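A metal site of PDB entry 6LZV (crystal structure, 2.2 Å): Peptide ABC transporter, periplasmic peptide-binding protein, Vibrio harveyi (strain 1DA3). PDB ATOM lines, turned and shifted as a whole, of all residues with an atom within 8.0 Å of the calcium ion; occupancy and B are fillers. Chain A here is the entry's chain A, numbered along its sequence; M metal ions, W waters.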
ATOM      1  N   LYS A 339      19.822  22.379   8.584  1.00  0.00           N
ATOM      2  CA  LYS A 339      19.903  20.928   8.530  1.00  0.00           C
ATOM      3  C   LYS A 339      19.128  20.253   9.673  1.00  0.00           C
ATOM      4  O   LYS A 339      19.285  20.650  10.818  1.00  0.00           O
ATOM      5  CB  LYS A 339      21.364  20.513   8.620  1.00  0.00           C
ATOM      6  CG  LYS A 339      21.600  19.001   8.491  1.00  0.00           C
ATOM      7  CD  LYS A 339      23.093  18.698   8.569  1.00  0.00           C
ATOM      8  CE  LYS A 339      23.381  17.186   8.689  1.00  0.00           C
ATOM      9  NZ  LYS A 339      24.841  16.945   8.979  1.00  0.00           N
ATOM     10  N   ASP A 340      18.360  19.207   9.383  1.00  0.00           N
ATOM     11  CA  ASP A 340      17.690  18.444  10.451  1.00  0.00           C
ATOM     12  C   ASP A 340      18.702  17.622  11.217  1.00  0.00           C
ATOM     13  O   ASP A 340      19.216  16.628  10.720  1.00  0.00           O
ATOM     14  CB  ASP A 340      16.613  17.506   9.872  1.00  0.00           C
ATOM     15  CG  ASP A 340      15.914  16.644  10.968  1.00  0.00           C
ATOM     16  OD1 ASP A 340      15.955  16.987  12.153  1.00  0.00           O
ATOM     17  OD2 ASP A 340      15.306  15.608  10.621  1.00  0.00           O
ATOM     18  N   VAL A 341      18.985  17.998  12.456  1.00  0.00           N
ATOM     19  CA  VAL A 341      19.991  17.221  13.181  1.00  0.00           C
ATOM     20  C   VAL A 341      19.452  16.418  14.357  1.00  0.00           C
ATOM     21  O   VAL A 341      20.242  15.938  15.160  1.00  0.00           O
ATOM     22  CB  VAL A 341      21.107  18.143  13.692  1.00  0.00           C
ATOM     23  CG1 VAL A 341      21.997  18.581  12.514  1.00  0.00           C
ATOM     24  CG2 VAL A 341      20.509  19.344  14.420  1.00  0.00           C
ATOM     25  N   ASN A 342      18.140  16.276  14.474  1.00  0.00           N
ATOM     26  CA  ASN A 342      17.580  15.453  15.560  1.00  0.00           C
ATOM     27  C   ASN A 342      16.499  14.501  15.046  1.00  0.00           C
ATOM     28  O   ASN A 342      15.591  14.133  15.773  1.00  0.00           O
ATOM     29  CB  ASN A 342      17.044  16.333  16.699  1.00  0.00           C
ATOM     30  CG  ASN A 342      15.799  17.114  16.298  1.00  0.00           C
ATOM     31  OD1 ASN A 342      15.488  17.227  15.109  1.00  0.00           O
ATOM     32  ND2 ASN A 342      15.080  17.641  17.283  1.00  0.00           N
ATOM     33  N   LYS A 343      16.629  14.137  13.780  1.00  0.00           N
ATOM     34  CA  LYS A 343      15.829  13.070  13.158  1.00  0.00           C
ATOM     35  C   LYS A 343      14.310  13.188  13.257  1.00  0.00           C
ATOM     36  O   LYS A 343      13.633  12.160  13.374  1.00  0.00           O
ATOM     37  CB  LYS A 343      16.222  11.715  13.744  1.00  0.00           C
ATOM     38  CG  LYS A 343      17.697  11.483  13.860  1.00  0.00           C
ATOM     39  CD  LYS A 343      17.973  10.051  14.282  1.00  0.00           C
ATOM     40  CE  LYS A 343      19.128  10.002  15.268  1.00  0.00           C
ATOM     41  NZ  LYS A 343      20.401  10.377  14.634  1.00  0.00           N
ATOM     42  N   ASP A 344      13.741  14.383  13.192  1.00  0.00           N
ATOM     43  CA  ASP A 344      12.290  14.476  13.223  1.00  0.00           C
ATOM     44  C   ASP A 344      11.754  14.927  11.877  1.00  0.00           C
ATOM     45  O   ASP A 344      10.549  15.119  11.727  1.00  0.00           O
ATOM     46  CB  ASP A 344      11.809  15.397  14.338  1.00  0.00           C
ATOM     47  CG  ASP A 344      12.188  16.841  14.121  1.00  0.00           C
ATOM     48  OD1 ASP A 344      13.080  17.119  13.264  1.00  0.00           O
ATOM     49  OD2 ASP A 344      11.605  17.701  14.802  1.00  0.00           O
ATOM     50  N   GLY A 345      12.642  15.092  10.895  1.00  0.00           N
ATOM     51  CA  GLY A 345      12.239  15.511   9.562  1.00  0.00           C
ATOM     52  C   GLY A 345      12.038  17.012   9.392  1.00  0.00           C
ATOM     53  O   GLY A 345      11.704  17.495   8.298  1.00  0.00           O
ATOM     54  N   PHE A 346      12.229  17.769  10.455  1.00  0.00           N
ATOM     55  CA  PHE A 346      12.124  19.219  10.347  1.00  0.00           C
ATOM     56  C   PHE A 346      13.497  19.878  10.484  1.00  0.00           C
ATOM     57  O   PHE A 346      14.287  19.481  11.344  1.00  0.00           O
ATOM     58  CB  PHE A 346      11.164  19.753  11.409  1.00  0.00           C
ATOM     59  CG  PHE A 346       9.739  19.342  11.175  1.00  0.00           C
ATOM     60  CD1 PHE A 346       9.023  19.877  10.103  1.00  0.00           C
ATOM     61  CD2 PHE A 346       9.131  18.401  11.976  1.00  0.00           C
ATOM     62  CE1 PHE A 346       7.716  19.493   9.856  1.00  0.00           C
ATOM     63  CE2 PHE A 346       7.823  18.026  11.735  1.00  0.00           C
ATOM     64  CZ  PHE A 346       7.121  18.561  10.665  1.00  0.00           C
ATOM     65  N   VAL A 347      13.785  20.867   9.638  1.00  0.00           N
ATOM     66  CA  VAL A 347      15.100  21.479   9.647  1.00  0.00           C
ATOM     67  C   VAL A 347      15.318  22.260  10.936  1.00  0.00           C
ATOM     68  O   VAL A 347      14.405  22.850  11.500  1.00  0.00           O
ATOM     69  CB  VAL A 347      15.360  22.419   8.436  1.00  0.00           C
ATOM     70  CG1 VAL A 347      15.197  21.671   7.118  1.00  0.00           C
ATOM     71  CG2 VAL A 347      14.431  23.611   8.471  1.00  0.00           C
ATOM     72  N   ASP A 348      16.569  22.254  11.392  1.00  0.00           N
ATOM     73  CA  ASP A 348      16.962  22.995  12.573  1.00  0.00           C
ATOM     74  C   ASP A 348      17.870  24.174  12.161  1.00  0.00           C
ATOM     75  O   ASP A 348      18.329  24.229  11.032  1.00  0.00           O
ATOM     76  CB  ASP A 348      17.631  22.033  13.537  1.00  0.00           C
ATOM     77  CG  ASP A 348      16.736  20.789  13.821  1.00  0.00           C
ATOM     78  OD1 ASP A 348      15.567  20.981  14.241  1.00  0.00           O
ATOM     79  OD2 ASP A 348      17.190  19.632  13.582  1.00  0.00           O
ATOM     80  N   THR A 349      18.087  25.140  13.045  1.00  0.00           N
ATOM     81  CA  THR A 349      18.878  26.323  12.690  1.00  0.00           C
ATOM     82  C   THR A 349      20.345  25.940  12.443  1.00  0.00           C
ATOM     83  O   THR A 349      20.768  24.857  12.838  1.00  0.00           O
ATOM     84  CB  THR A 349      18.838  27.396  13.798  1.00  0.00           C
ATOM     85  OG1 THR A 349      19.581  26.919  14.934  1.00  0.00           O
ATOM     86  CG2 THR A 349      17.422  27.724  14.212  1.00  0.00           C
ATOM     87  N   GLY A 352      22.105  24.425  15.288  1.00  0.00           N
ATOM     88  CA  GLY A 352      21.630  23.121  15.711  1.00  0.00           C
ATOM     89  C   GLY A 352      20.319  23.109  16.492  1.00  0.00           C
ATOM     90  O   GLY A 352      19.933  22.066  16.975  1.00  0.00           O
ATOM     91  N   LYS A 353      19.642  24.253  16.602  1.00  0.00           N
ATOM     92  CA  LYS A 353      18.445  24.353  17.443  1.00  0.00           C
ATOM     93  C   LYS A 353      17.147  24.049  16.715  1.00  0.00           C
ATOM     94  O   LYS A 353      16.934  24.541  15.623  1.00  0.00           O
ATOM     95  CB  LYS A 353      18.316  25.756  18.041  1.00  0.00           C
ATOM     96  CG  LYS A 353      19.458  26.189  18.949  1.00  0.00           C
ATOM     97  CD  LYS A 353      19.201  27.613  19.453  1.00  0.00           C
ATOM     98  CE  LYS A 353      20.296  28.115  20.394  1.00  0.00           C
ATOM     99  NZ  LYS A 353      21.559  28.389  19.634  1.00  0.00           N
ATOM    100  N   SER A 354      16.284  23.240  17.333  1.00  0.00           N
ATOM    101  CA  SER A 354      14.955  22.953  16.791  1.00  0.00           C
ATOM    102  C   SER A 354      14.076  24.139  17.005  1.00  0.00           C
ATOM    103  O   SER A 354      14.281  24.913  17.940  1.00  0.00           O
ATOM    104  CB  SER A 354      14.313  21.727  17.462  1.00  0.00           C
ATOM    105  OG  SER A 354      15.010  20.547  17.094  1.00  0.00           O
ATOM    106  N   PHE A 355      13.082  24.295  16.135  1.00  0.00           N
ATOM    107  CA  PHE A 355      12.151  25.388  16.303  1.00  0.00           C
ATOM    108  C   PHE A 355      10.877  25.136  15.567  1.00  0.00           C
ATOM    109  O   PHE A 355      10.812  24.384  14.612  1.00  0.00           O
ATOM    110  CB  PHE A 355      12.763  26.715  15.835  1.00  0.00           C
ATOM    111  CG  PHE A 355      13.070  26.758  14.365  1.00  0.00           C
ATOM    112  CD1 PHE A 355      14.216  26.149  13.864  1.00  0.00           C
ATOM    113  CD2 PHE A 355      12.203  27.393  13.482  1.00  0.00           C
ATOM    114  CE1 PHE A 355      14.492  26.176  12.496  1.00  0.00           C
ATOM    115  CE2 PHE A 355      12.480  27.436  12.107  1.00  0.00           C
ATOM    116  CZ  PHE A 355      13.630  26.817  11.625  1.00  0.00           C
ATOM    117  N   GLY A 383      10.020  20.707   5.057  1.00  0.00           N
ATOM    118  CA  GLY A 383      10.725  20.476   6.322  1.00  0.00           C
ATOM    119  C   GLY A 383      10.813  21.670   7.274  1.00  0.00           C
ATOM    120  O   GLY A 383      11.682  21.723   8.145  1.00  0.00           O
ATOM    121  N   LYS A 385       8.856  23.470  10.274  1.00  0.00           N
ATOM    122  CA  LYS A 385       7.769  23.170  11.183  1.00  0.00           C
ATOM    123  C   LYS A 385       7.076  24.448  11.624  1.00  0.00           C
ATOM    124  O   LYS A 385       7.711  25.400  12.060  1.00  0.00           O
ATOM    125  CB  LYS A 385       8.271  22.401  12.395  1.00  0.00           C
ATOM    126  CG  LYS A 385       7.151  21.881  13.262  1.00  0.00           C
ATOM    127  CD  LYS A 385       7.688  21.529  14.616  1.00  0.00           C
ATOM    128  CE  LYS A 385       7.317  20.121  15.054  1.00  0.00           C
ATOM    129  NZ  LYS A 385       8.192  19.728  16.221  1.00  0.00           N
HETATM  130 CA    CA M   1      14.894  18.710  13.443  1.00  0.00          CA
HETATM  131  O   HOH W   1      13.234  19.697  14.589  1.00  0.00           O
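The calcium ion is bound by water W1 (2.2 Å), the side-chain amide oxygen (OD1) of Asn 342 (2.3 Å), the backbone carbonyl oxygen (O) of Phe 346 (2.3 Å), the side-chain carboxylate (OD1) of Asp 340 (2.4 Å), the side-chain carboxylate (OD1) of Asp 344 (2.4 Å), the side-chain carboxylate (OD2) of Asp 348 (2.5 Å) and the side-chain carboxylate (OD1) of Asp 348 (2.5 Å).
The nearest printed residue that does not touch the calcium ion is Ser 354 (4.1 Å).
ND2 of Asn 342 is in hydrogen-bond range of OG of Ser 354 (2.9 Å).
OD1 of Asp 340 lies close to N of Lys 343 (3.4 Å).
N of Gly 345 lies within hydrogen-bond range of OD2 of Asp 340, 2.7 Å away.
The side-chain hydroxyl (OG) of Ser 354 lies close to the side-chain carboxylate (OD1) of Asp 348 (2.9 Å).
The side-chain carboxylate of Asp 348 lies close to the backbone NH of Val 341 (2.7 Å).
The backbone carbonyl oxygen (O) of Lys 339 sits at hydrogen-bond distance from the backbone NH (N) of Asp 348, at 3.2 Å.
Water W1 lies within hydrogen-bond range of OD2 of Asp 344 (2.6 Å) and OG of Ser 354 (3.2 Å).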
